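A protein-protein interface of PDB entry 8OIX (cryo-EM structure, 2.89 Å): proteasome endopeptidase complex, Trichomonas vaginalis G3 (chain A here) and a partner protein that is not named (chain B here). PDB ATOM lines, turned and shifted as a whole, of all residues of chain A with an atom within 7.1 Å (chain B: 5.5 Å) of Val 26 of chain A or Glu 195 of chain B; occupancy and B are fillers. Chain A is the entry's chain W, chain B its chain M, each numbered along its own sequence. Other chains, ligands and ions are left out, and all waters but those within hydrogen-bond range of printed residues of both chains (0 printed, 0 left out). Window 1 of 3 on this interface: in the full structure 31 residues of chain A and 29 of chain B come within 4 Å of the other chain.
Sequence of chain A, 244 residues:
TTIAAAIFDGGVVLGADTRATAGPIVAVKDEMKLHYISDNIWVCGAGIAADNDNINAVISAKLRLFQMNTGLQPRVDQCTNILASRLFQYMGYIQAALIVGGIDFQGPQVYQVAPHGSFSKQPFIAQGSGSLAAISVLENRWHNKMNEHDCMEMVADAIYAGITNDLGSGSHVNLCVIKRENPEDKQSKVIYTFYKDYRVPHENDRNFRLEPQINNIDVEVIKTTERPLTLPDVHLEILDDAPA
SG of Cys 191 of chain B is in hydrogen-bond range of OD1 of Asn 207 of chain A. The side-chain hydroxyl (OG) of Ser 192 of chain B lies within hydrogen-bond range of the guanidinium group (NH2) of Arg 206 of chain A (3.0 Å). NZ of Lys 29 of chain A is in salt-bridge range of OE1 of Glu 195 of chain B, at 2.5 Å. The guanidinium group (NH1) of Arg 196 of chain B lies within hydrogen-bond range of the backbone carbonyl oxygen (O) of Val 26 of chain A, at 2.7 Å. The backbone carbonyl oxygen (O) of Ala 27 of chain A sits at hydrogen-bond distance from the guanidinium group (NH1) of Arg 196 of chain B. The backbone NH of Ile 198 of chain B is in hydrogen-bond range of the backbone carbonyl oxygen of Pro 24 of chain A (3.0 Å). The guanidinium group (NH1) of Arg 19 of chain A lies within salt-bridge range of the chain-end carboxylate (O) of His 224 of chain B, 2.7 Å away. The side-chain amide oxygen (OD1) of Asn 204 of chain A is in hydrogen-bond range of the backbone NH (N) of His 224 of chain B, at 3.2 Å. The backbone carbonyl oxygen (O) of Pro 24 of chain A sits close to the side-chain carboxylate (OD1) of Asp 197 of chain B. The backbone carbonyl oxygen (O) of Ser 169 of chain A sits close to the chain-end carboxylate (O) of His 224 of chain B (3.1 Å).
The backbone NH (N) of Thr 18 of chain A sits at hydrogen-bond distance from the backbone carbonyl oxygen (O) of Gly 170 of chain A (3.4 Å). The side-chain hydroxyl (OG1) of Thr 18 of chain A is in hydrogen-bond range of the side-chain hydroxyl (OG) of Ser 171 of chain A. N of Arg 19 of chain A lies within hydrogen-bond range of OG of Ser 171 of chain A (3.2 Å). N of Ala 27 of chain A sits at hydrogen-bond distance from O of Ala 20 of chain A (2.8 Å). OG1 of Thr 21 of chain A sits close to O of Gly 23 of chain A. The backbone carbonyl oxygen (O) of Lys 29 of chain A lies close to the side-chain hydroxyl (OG) of Ser 171 of chain A, at 3.4 Å.
Among the printed residues, pairs that only touch across the chains: Thr 21 of chain A with Ile 198 of chain B (3.7 Å), Pro 24 of chain A with Arg 196 of chain B (3.9 Å), Ile 25 of chain A with Arg 196 of chain B (3.2 Å), Ile 25 of chain A with Asp 197 of chain B (3.97 Å), Val 26 of chain A with Glu 195 of chain B (3.5 Å), Val 26 of chain A with Ile 198 of chain B (3.5 Å), Leu 167 of chain A with Ile 198 of chain B (3.5 Å), Gly 170 of chain A with His 224 of chain B (3.6 Å), Ser 171 of chain A with His 224 of chain B (3.1 Å), Asn 204 of chain A with Glu 195 of chain B (3.9 Å), Asn 204 of chain A with Pro 222 of chain B (3.3 Å), Asp 205 of chain A with Glu 195 of chain B (3.96 Å), Asp 205 of chain A with Pro 222 of chain B (3.2 Å), Arg 206 of chain A with Cys 191 of chain B (3.3 Å), Arg 206 of chain A with Glu 195 of chain B (3.7 Å) and Asn 207 of chain A with Pro 222 of chain B (3.8 Å).
Of chain B, only Glu 195 (3.5 Å), Arg 196 (2.4 Å) and Ile 198 (3.5 Å) come within 4 Å of Val 26 of chain A. Glu 195 of chain B touches just these residues of chain A: Val 26, Lys 29, Asn 204, Asp 205 and Arg 206. Printed residues of chain B within 4 Å of Asp 205 of chain A: Glu 195 and Pro 222. Printed residues of chain A within 4 Å of Ser 192 of chain B: Arg 206 (3.0 Å). Of the printed residues of chain B, Pro 24 of chain A touches Arg 196, Asp 197 and Ile 198. The nearest residue of chain B that does not touch Val 26 of chain A is Asp 197 of chain B (4.6 Å).
Of the 23 printed residues of chain A, 15 touch a printed residue of chain B. Printed residues of chain A that touch a printed residue of chain B: Arg 19, Thr 21, Pro 24, Ile 25, Val 26, Ala 27, Lys 29, Leu 167, Ser 169, Gly 170, Ser 171, Asn 204, Asp 205, Arg 206 and Asn 207. Hydrophobic or aromatic side chains of chain A within 4 Å of the printed part of chain B: Ile 25, Val 26 and Leu 167. Of the 11 printed residues of chain B, 8 touch a printed residue of chain A. Printed residues of chain B that touch a printed residue of chain A: Cys 191, Ser 192, Glu 195, Arg 196, Asp 197, Ile 198, Pro 222 and His 224. Along chain B the printed residues that touch a printed residue of chain A span positions 191 to 224. Among the printed residues, 26 pairs touch across the chains. Among the printed residues, Asp or Glu carboxylates within 4 Å of a Lys or Arg side-chain nitrogen of the other chain: Lys 29 of chain A with Glu 195 of chain B (2.5 Å).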
ATOM      1  N   THR A  18     -10.452   9.267  17.852  1.00  0.00           N
ATOM      2  CA  THR A  18     -11.114   9.931  18.973  1.00  0.00           C
ATOM      3  C   THR A  18     -10.082  10.407  19.958  1.00  0.00           C
ATOM      4  O   THR A  18     -10.382  10.417  21.156  1.00  0.00           O
ATOM      5  CB  THR A  18     -12.076   8.911  19.564  1.00  0.00           C
ATOM      6  OG1 THR A  18     -11.266   7.787  19.883  1.00  0.00           O
ATOM      7  CG2 THR A  18     -13.154   8.490  18.588  1.00  0.00           C
ATOM      8  N   ARG A  19      -8.905  10.801  19.476  1.00  0.00           N
ATOM      9  CA  ARG A  19      -7.816  11.227  20.386  1.00  0.00           C
ATOM     10  C   ARG A  19      -7.534  12.717  20.220  1.00  0.00           C
ATOM     11  O   ARG A  19      -7.133  13.126  19.114  1.00  0.00           O
ATOM     12  CB  ARG A  19      -6.493  10.523  20.089  1.00  0.00           C
ATOM     13  CG  ARG A  19      -5.290  11.121  20.802  1.00  0.00           C
ATOM     14  CD  ARG A  19      -3.988  10.454  20.416  1.00  0.00           C
ATOM     15  NE  ARG A  19      -3.837   9.145  21.058  1.00  0.00           N
ATOM     16  CZ  ARG A  19      -2.691   8.491  21.121  1.00  0.00           C
ATOM     17  NH1 ARG A  19      -1.914   8.427  20.061  1.00  0.00           N
ATOM     18  NH2 ARG A  19      -2.317   7.909  22.245  1.00  0.00           N
ATOM     19  N   ALA A  20      -7.744  13.500  21.272  1.00  0.00           N
ATOM     20  CA  ALA A  20      -7.353  14.922  21.216  1.00  0.00           C
ATOM     21  C   ALA A  20      -6.124  15.077  22.107  1.00  0.00           C
ATOM     22  O   ALA A  20      -6.159  14.571  23.237  1.00  0.00           O
ATOM     23  CB  ALA A  20      -8.489  15.784  21.675  1.00  0.00           C
ATOM     24  N   THR A  21      -5.062  15.705  21.603  1.00  0.00           N
ATOM     25  CA  THR A  21      -3.840  15.841  22.382  1.00  0.00           C
ATOM     26  C   THR A  21      -3.611  17.301  22.742  1.00  0.00           C
ATOM     27  O   THR A  21      -3.715  18.182  21.884  1.00  0.00           O
ATOM     28  CB  THR A  21      -2.623  15.298  21.628  1.00  0.00           C
ATOM     29  OG1 THR A  21      -2.462  16.002  20.394  1.00  0.00           O
ATOM     30  CG2 THR A  21      -2.792  13.823  21.340  1.00  0.00           C
ATOM     31  N   ALA A  22      -3.306  17.547  24.011  1.00  0.00           N
ATOM     32  CA  ALA A  22      -2.919  18.877  24.477  1.00  0.00           C
ATOM     33  C   ALA A  22      -1.397  18.998  24.471  1.00  0.00           C
ATOM     34  O   ALA A  22      -0.742  19.176  25.497  1.00  0.00           O
ATOM     35  CB  ALA A  22      -3.497  19.141  25.864  1.00  0.00           C
ATOM     36  N   GLY A  23      -0.841  18.892  23.267  1.00  0.00           N
ATOM     37  CA  GLY A  23       0.586  18.803  23.082  1.00  0.00           C
ATOM     38  C   GLY A  23       1.012  17.363  22.888  1.00  0.00           C
ATOM     39  O   GLY A  23       0.455  16.636  22.061  1.00  0.00           O
ATOM     40  N   PRO A  24       2.016  16.918  23.645  1.00  0.00           N
ATOM     41  CA  PRO A  24       2.411  15.506  23.615  1.00  0.00           C
ATOM     42  C   PRO A  24       1.579  14.600  24.507  1.00  0.00           C
ATOM     43  O   PRO A  24       1.888  13.410  24.607  1.00  0.00           O
ATOM     44  CB  PRO A  24       3.864  15.560  24.108  1.00  0.00           C
ATOM     45  CG  PRO A  24       3.897  16.729  25.017  1.00  0.00           C
ATOM     46  CD  PRO A  24       2.932  17.737  24.458  1.00  0.00           C
ATOM     47  N   ILE A  25       0.539  15.124  25.150  1.00  0.00           N
ATOM     48  CA  ILE A  25      -0.266  14.385  26.115  1.00  0.00           C
ATOM     49  C   ILE A  25      -1.668  14.215  25.549  1.00  0.00           C
ATOM     50  O   ILE A  25      -2.228  15.150  24.966  1.00  0.00           O
ATOM     51  CB  ILE A  25      -0.293  15.103  27.481  1.00  0.00           C
ATOM     52  CG1 ILE A  25       0.828  14.587  28.388  1.00  0.00           C
ATOM     53  CG2 ILE A  25      -1.644  14.946  28.164  1.00  0.00           C
ATOM     54  CD1 ILE A  25       2.225  14.879  27.893  1.00  0.00           C
ATOM     55  N   VAL A  26      -2.240  13.026  25.729  1.00  0.00           N
ATOM     56  CA  VAL A  26      -3.552  12.701  25.181  1.00  0.00           C
ATOM     57  C   VAL A  26      -4.586  13.270  26.145  1.00  0.00           C
ATOM     58  O   VAL A  26      -4.910  12.660  27.167  1.00  0.00           O
ATOM     59  CB  VAL A  26      -3.735  11.196  24.983  1.00  0.00           C
ATOM     60  CG1 VAL A  26      -5.141  10.894  24.498  1.00  0.00           C
ATOM     61  CG2 VAL A  26      -2.719  10.666  24.003  1.00  0.00           C
ATOM     62  N   ALA A  27      -5.093  14.460  25.824  1.00  0.00           N
ATOM     63  CA  ALA A  27      -6.104  15.090  26.663  1.00  0.00           C
ATOM     64  C   ALA A  27      -7.403  14.296  26.652  1.00  0.00           C
ATOM     65  O   ALA A  27      -7.997  14.040  27.705  1.00  0.00           O
ATOM     66  CB  ALA A  27      -6.346  16.525  26.199  1.00  0.00           C
ATOM     67  N   VAL A  28      -7.860  13.891  25.468  1.00  0.00           N
ATOM     68  CA  VAL A  28      -9.137  13.208  25.308  1.00  0.00           C
ATOM     69  C   VAL A  28      -8.909  11.891  24.585  1.00  0.00           C
ATOM     70  O   VAL A  28      -8.133  11.823  23.626  1.00  0.00           O
ATOM     71  CB  VAL A  28     -10.150  14.070  24.527  1.00  0.00           C
ATOM     72  CG1 VAL A  28     -11.567  13.572  24.764  1.00  0.00           C
ATOM     73  CG2 VAL A  28     -10.006  15.529  24.894  1.00  0.00           C
ATOM     74  N   LYS A  29      -9.593  10.844  25.041  1.00  0.00           N
ATOM     75  CA  LYS A  29      -9.531   9.537  24.405  1.00  0.00           C
ATOM     76  C   LYS A  29     -10.860   9.138  23.781  1.00  0.00           C
ATOM     77  O   LYS A  29     -10.977   8.028  23.251  1.00  0.00           O
ATOM     78  CB  LYS A  29      -9.080   8.477  25.415  1.00  0.00           C
ATOM     79  CG  LYS A  29      -7.745   8.796  26.071  1.00  0.00           C
ATOM     80  CD  LYS A  29      -7.198   7.611  26.844  1.00  0.00           C
ATOM     81  CE  LYS A  29      -8.143   7.185  27.950  1.00  0.00           C
ATOM     82  NZ  LYS A  29      -7.646   5.970  28.651  1.00  0.00           N
ATOM     83  N   ASP A  30     -11.862  10.016  23.832  1.00  0.00           N
ATOM     84  CA  ASP A  30     -13.165   9.804  23.216  1.00  0.00           C
ATOM     85  C   ASP A  30     -13.603  11.054  22.466  1.00  0.00           C
ATOM     86  O   ASP A  30     -14.801  11.307  22.312  1.00  0.00           O
ATOM     87  CB  ASP A  30     -14.211   9.402  24.257  1.00  0.00           C
ATOM     88  CG  ASP A  30     -14.403  10.456  25.327  1.00  0.00           C
ATOM     89  OD1 ASP A  30     -13.420  10.777  26.027  1.00  0.00           O
ATOM     90  OD2 ASP A  30     -15.535  10.964  25.466  1.00  0.00           O
ATOM     91  N   LEU A 167       1.217   9.374  16.169  1.00  0.00           N
ATOM     92  CA  LEU A 167       1.088   9.582  17.607  1.00  0.00           C
ATOM     93  C   LEU A 167      -0.054  10.535  17.937  1.00  0.00           C
ATOM     94  O   LEU A 167      -0.730  10.365  18.957  1.00  0.00           O
ATOM     95  CB  LEU A 167       2.400  10.107  18.180  1.00  0.00           C
ATOM     96  CG  LEU A 167       3.618   9.248  17.857  1.00  0.00           C
ATOM     97  CD1 LEU A 167       4.876   9.865  18.425  1.00  0.00           C
ATOM     98  CD2 LEU A 167       3.400   7.872  18.425  1.00  0.00           C
ATOM     99  N   GLY A 168      -0.279  11.540  17.093  1.00  0.00           N
ATOM    100  CA  GLY A 168      -1.390  12.452  17.298  1.00  0.00           C
ATOM    101  C   GLY A 168      -2.756  11.822  17.132  1.00  0.00           C
ATOM    102  O   GLY A 168      -3.753  12.443  17.512  1.00  0.00           O
ATOM    103  N   SER A 169      -2.824  10.617  16.576  1.00  0.00           N
ATOM    104  CA  SER A 169      -4.068   9.881  16.422  1.00  0.00           C
ATOM    105  C   SER A 169      -4.056   8.637  17.297  1.00  0.00           C
ATOM    106  O   SER A 169      -3.001   8.053  17.560  1.00  0.00           O
ATOM    107  CB  SER A 169      -4.286   9.473  14.965  1.00  0.00           C
ATOM    108  OG  SER A 169      -4.002  10.545  14.087  1.00  0.00           O
ATOM    109  N   GLY A 170      -5.236   8.236  17.749  1.00  0.00           N
ATOM    110  CA  GLY A 170      -5.333   7.031  18.544  1.00  0.00           C
ATOM    111  C   GLY A 170      -6.749   6.758  18.989  1.00  0.00           C
ATOM    112  O   GLY A 170      -7.708   7.329  18.468  1.00  0.00           O
ATOM    113  N   SER A 171      -6.858   5.869  19.973  1.00  0.00           N
ATOM    114  CA  SER A 171      -8.116   5.441  20.609  1.00  0.00           C
ATOM    115  C   SER A 171      -9.024   4.824  19.545  1.00  0.00           C
ATOM    116  O   SER A 171      -8.561   3.964  18.779  1.00  0.00           O
ATOM    117  CB  SER A 171      -8.719   6.595  21.402  1.00  0.00           C
ATOM    118  OG  SER A 171      -8.783   7.788  20.647  1.00  0.00           O
ATOM    119  N   ASN A 204      -4.854  -1.537  21.762  1.00  0.00           N
ATOM    120  CA  ASN A 204      -4.649  -0.147  22.139  1.00  0.00           C
ATOM    121  C   ASN A 204      -5.384   0.216  23.421  1.00  0.00           C
ATOM    122  O   ASN A 204      -5.496   1.402  23.747  1.00  0.00           O
ATOM    123  CB  ASN A 204      -5.093   0.772  20.999  1.00  0.00           C
ATOM    124  CG  ASN A 204      -4.234   0.621  19.761  1.00  0.00           C
ATOM    125  OD1 ASN A 204      -3.212  -0.061  19.782  1.00  0.00           O
ATOM    126  ND2 ASN A 204      -4.661   1.235  18.666  1.00  0.00           N
ATOM    127  N   ASP A 205      -5.888  -0.772  24.151  1.00  0.00           N
ATOM    128  CA  ASP A 205      -6.592  -0.541  25.400  1.00  0.00           C
ATOM    129  C   ASP A 205      -5.643  -0.661  26.588  1.00  0.00           C
ATOM    130  O   ASP A 205      -4.544  -1.211  26.486  1.00  0.00           O
ATOM    131  CB  ASP A 205      -7.751  -1.527  25.557  1.00  0.00           C
ATOM    132  CG  ASP A 205      -8.914  -1.208  24.640  1.00  0.00           C
ATOM    133  OD1 ASP A 205      -9.068  -0.027  24.263  1.00  0.00           O
ATOM    134  OD2 ASP A 205      -9.675  -2.138  24.299  1.00  0.00           O
ATOM    135  N   ARG A 206      -6.090  -0.138  27.728  1.00  0.00           N
ATOM    136  CA  ARG A 206      -5.358  -0.275  28.980  1.00  0.00           C
ATOM    137  C   ARG A 206      -5.286  -1.746  29.372  1.00  0.00           C
ATOM    138  O   ARG A 206      -6.290  -2.335  29.781  1.00  0.00           O
ATOM    139  CB  ARG A 206      -6.034   0.550  30.078  1.00  0.00           C
ATOM    140  CG  ARG A 206      -5.375   0.469  31.442  1.00  0.00           C
ATOM    141  CD  ARG A 206      -4.045   1.192  31.456  1.00  0.00           C
ATOM    142  NE  ARG A 206      -3.481   1.262  32.798  1.00  0.00           N
ATOM    143  CZ  ARG A 206      -3.583   2.313  33.600  1.00  0.00           C
ATOM    144  NH1 ARG A 206      -4.223   3.408  33.225  1.00  0.00           N
ATOM    145  NH2 ARG A 206      -3.026   2.264  34.806  1.00  0.00           N
ATOM    146  N   ASN A 207      -4.103  -2.344  29.252  1.00  0.00           N
ATOM    147  CA  ASN A 207      -3.944  -3.776  29.463  1.00  0.00           C
ATOM    148  C   ASN A 207      -3.531  -4.136  30.882  1.00  0.00           C
ATOM    149  O   ASN A 207      -3.564  -5.319  31.236  1.00  0.00           O
ATOM    150  CB  ASN A 207      -2.910  -4.343  28.489  1.00  0.00           C
ATOM    151  CG  ASN A 207      -1.593  -3.607  28.549  1.00  0.00           C
ATOM    152  OD1 ASN A 207      -1.552  -2.399  28.779  1.00  0.00           O
ATOM    153  ND2 ASN A 207      -0.501  -4.335  28.359  1.00  0.00           N
ATOM    154  N   ARG A 209      -3.531  -2.685  35.216  1.00  0.00           N
ATOM    155  CA  ARG A 209      -3.989  -1.742  36.224  1.00  0.00           C
ATOM    156  C   ARG A 209      -3.898  -2.391  37.597  1.00  0.00           C
ATOM    157  O   ARG A 209      -4.406  -3.499  37.797  1.00  0.00           O
ATOM    158  CB  ARG A 209      -5.422  -1.295  35.932  1.00  0.00           C
ATOM    159  CG  ARG A 209      -5.924  -0.187  36.835  1.00  0.00           C
ATOM    160  CD  ARG A 209      -7.300   0.282  36.407  1.00  0.00           C
ATOM    161  NE  ARG A 209      -7.279   0.909  35.091  1.00  0.00           N
ATOM    162  CZ  ARG A 209      -7.082   2.203  34.882  1.00  0.00           C
ATOM    163  NH1 ARG A 209      -6.864   3.039  35.883  1.00  0.00           N
ATOM    164  NH2 ARG A 209      -7.103   2.670  33.637  1.00  0.00           N
ATOM    165  N   ILE B 190       3.565   3.007  33.717  1.00  0.00           N
ATOM    166  CA  ILE B 190       3.906   3.028  32.299  1.00  0.00           C
ATOM    167  C   ILE B 190       2.650   2.918  31.449  1.00  0.00           C
ATOM    168  O   ILE B 190       2.547   3.544  30.391  1.00  0.00           O
ATOM    169  CB  ILE B 190       4.915   1.909  31.975  1.00  0.00           C
ATOM    170  CG1 ILE B 190       6.302   2.259  32.512  1.00  0.00           C
ATOM    171  CG2 ILE B 190       4.993   1.667  30.483  1.00  0.00           C
ATOM    172  CD1 ILE B 190       6.982   3.367  31.738  1.00  0.00           C
ATOM    173  N   CYS B 191       1.665   2.144  31.906  1.00  0.00           N
ATOM    174  CA  CYS B 191       0.414   2.036  31.163  1.00  0.00           C
ATOM    175  C   CYS B 191      -0.361   3.347  31.193  1.00  0.00           C
ATOM    176  O   CYS B 191      -0.936   3.756  30.178  1.00  0.00           O
ATOM    177  CB  CYS B 191      -0.432   0.896  31.727  1.00  0.00           C
ATOM    178  SG  CYS B 191       0.234  -0.754  31.437  1.00  0.00           S
ATOM    179  N   SER B 192      -0.381   4.025  32.342  1.00  0.00           N
ATOM    180  CA  SER B 192      -1.025   5.333  32.418  1.00  0.00           C
ATOM    181  C   SER B 192      -0.328   6.345  31.517  1.00  0.00           C
ATOM    182  O   SER B 192      -0.984   7.122  30.810  1.00  0.00           O
ATOM    183  CB  SER B 192      -1.038   5.823  33.865  1.00  0.00           C
ATOM    184  OG  SER B 192      -1.569   4.835  34.727  1.00  0.00           O
ATOM    185  N   VAL B 193       1.006   6.340  31.521  1.00  0.00           N
ATOM    186  CA  VAL B 193       1.760   7.235  30.648  1.00  0.00           C
ATOM    187  C   VAL B 193       1.451   6.929  29.189  1.00  0.00           C
ATOM    188  O   VAL B 193       1.227   7.835  28.379  1.00  0.00           O
ATOM    189  CB  VAL B 193       3.265   7.133  30.948  1.00  0.00           C
ATOM    190  CG1 VAL B 193       4.043   7.941  29.954  1.00  0.00           C
ATOM    191  CG2 VAL B 193       3.552   7.629  32.347  1.00  0.00           C
ATOM    192  N   THR B 194       1.426   5.642  28.833  1.00  0.00           N
ATOM    193  CA  THR B 194       1.091   5.246  27.470  1.00  0.00           C
ATOM    194  C   THR B 194      -0.296   5.745  27.094  1.00  0.00           C
ATOM    195  O   THR B 194      -0.519   6.204  25.968  1.00  0.00           O
ATOM    196  CB  THR B 194       1.177   3.727  27.337  1.00  0.00           C
ATOM    197  OG1 THR B 194       2.540   3.311  27.477  1.00  0.00           O
ATOM    198  CG2 THR B 194       0.649   3.275  25.988  1.00  0.00           C
ATOM    199  N   GLU B 195      -1.238   5.675  28.035  1.00  0.00           N
ATOM    200  CA  GLU B 195      -2.582   6.175  27.782  1.00  0.00           C
ATOM    201  C   GLU B 195      -2.575   7.678  27.555  1.00  0.00           C
ATOM    202  O   GLU B 195      -3.383   8.190  26.772  1.00  0.00           O
ATOM    203  CB  GLU B 195      -3.505   5.827  28.950  1.00  0.00           C
ATOM    204  CG  GLU B 195      -3.935   4.375  29.003  1.00  0.00           C
ATOM    205  CD  GLU B 195      -4.785   3.985  27.811  1.00  0.00           C
ATOM    206  OE1 GLU B 195      -5.853   4.600  27.617  1.00  0.00           O
ATOM    207  OE2 GLU B 195      -4.386   3.067  27.067  1.00  0.00           O
ATOM    208  N   ARG B 196      -1.675   8.398  28.221  1.00  0.00           N
ATOM    209  CA  ARG B 196      -1.653   9.853  28.132  1.00  0.00           C
ATOM    210  C   ARG B 196      -0.535  10.393  27.246  1.00  0.00           C
ATOM    211  O   ARG B 196      -0.786  11.260  26.406  1.00  0.00           O
ATOM    212  CB  ARG B 196      -1.559  10.453  29.537  1.00  0.00           C
ATOM    213  CG  ARG B 196      -2.791  10.173  30.374  1.00  0.00           C
ATOM    214  CD  ARG B 196      -3.986  10.924  29.816  1.00  0.00           C
ATOM    215  NE  ARG B 196      -5.255  10.390  30.295  1.00  0.00           N
ATOM    216  CZ  ARG B 196      -6.440  10.896  29.986  1.00  0.00           C
ATOM    217  NH1 ARG B 196      -6.556  11.961  29.212  1.00  0.00           N
ATOM    218  NH2 ARG B 196      -7.537  10.314  30.461  1.00  0.00           N
ATOM    219  N   ASP B 197       0.697   9.920  27.414  1.00  0.00           N
ATOM    220  CA  ASP B 197       1.793  10.352  26.552  1.00  0.00           C
ATOM    221  C   ASP B 197       1.720   9.634  25.210  1.00  0.00           C
ATOM    222  O   ASP B 197       1.705   8.399  25.161  1.00  0.00           O
ATOM    223  CB  ASP B 197       3.139  10.090  27.220  1.00  0.00           C
ATOM    224  CG  ASP B 197       4.296  10.680  26.445  1.00  0.00           C
ATOM    225  OD1 ASP B 197       4.378  11.922  26.349  1.00  0.00           O
ATOM    226  OD2 ASP B 197       5.130   9.902  25.937  1.00  0.00           O
ATOM    227  N   ILE B 198       1.665  10.407  24.123  1.00  0.00           N
ATOM    228  CA  ILE B 198       1.622   9.813  22.789  1.00  0.00           C
ATOM    229  C   ILE B 198       2.916   9.061  22.493  1.00  0.00           C
ATOM    230  O   ILE B 198       2.898   7.979  21.895  1.00  0.00           O
ATOM    231  CB  ILE B 198       1.322  10.892  21.727  1.00  0.00           C
ATOM    232  CG1 ILE B 198       2.484  11.873  21.574  1.00  0.00           C
ATOM    233  CG2 ILE B 198       0.063  11.649  22.081  1.00  0.00           C
ATOM    234  CD1 ILE B 198       2.225  12.976  20.579  1.00  0.00           C
ATOM    235  N   PRO B 222      -0.678  -0.153  24.774  1.00  0.00           N
ATOM    236  CA  PRO B 222      -1.408   0.453  23.651  1.00  0.00           C
ATOM    237  C   PRO B 222      -0.518   1.053  22.570  1.00  0.00           C
ATOM    238  O   PRO B 222       0.225   2.007  22.818  1.00  0.00           O
ATOM    239  CB  PRO B 222      -2.242   1.536  24.337  1.00  0.00           C
ATOM    240  CG  PRO B 222      -2.447   1.043  25.709  1.00  0.00           C
ATOM    241  CD  PRO B 222      -1.274   0.193  26.076  1.00  0.00           C
ATOM    242  N   HIS B 224      -1.513   2.665  19.772  1.00  0.00           N
ATOM    243  CA  HIS B 224      -2.057   3.943  19.292  1.00  0.00           C
ATOM    244  C   HIS B 224      -1.284   5.168  19.782  1.00  0.00           C
ATOM    245  O   HIS B 224      -1.024   6.096  19.017  1.00  0.00           O
ATOM    246  CB  HIS B 224      -3.539   4.076  19.662  1.00  0.00           C
ATOM    247  CG  HIS B 224      -3.802   4.403  21.097  1.00  0.00           C
ATOM    248  ND1 HIS B 224      -3.662   3.486  22.116  1.00  0.00           N
ATOM    249  CD2 HIS B 224      -4.257   5.538  21.675  1.00  0.00           C
ATOM    250  CE1 HIS B 224      -3.986   4.056  23.263  1.00  0.00           C
ATOM    251  NE2 HIS B 224      -4.348   5.301  23.024  1.00  0.00           N
ATOM    252  OXT HIS B 224      -0.903   5.260  20.948  1.00  0.00           O
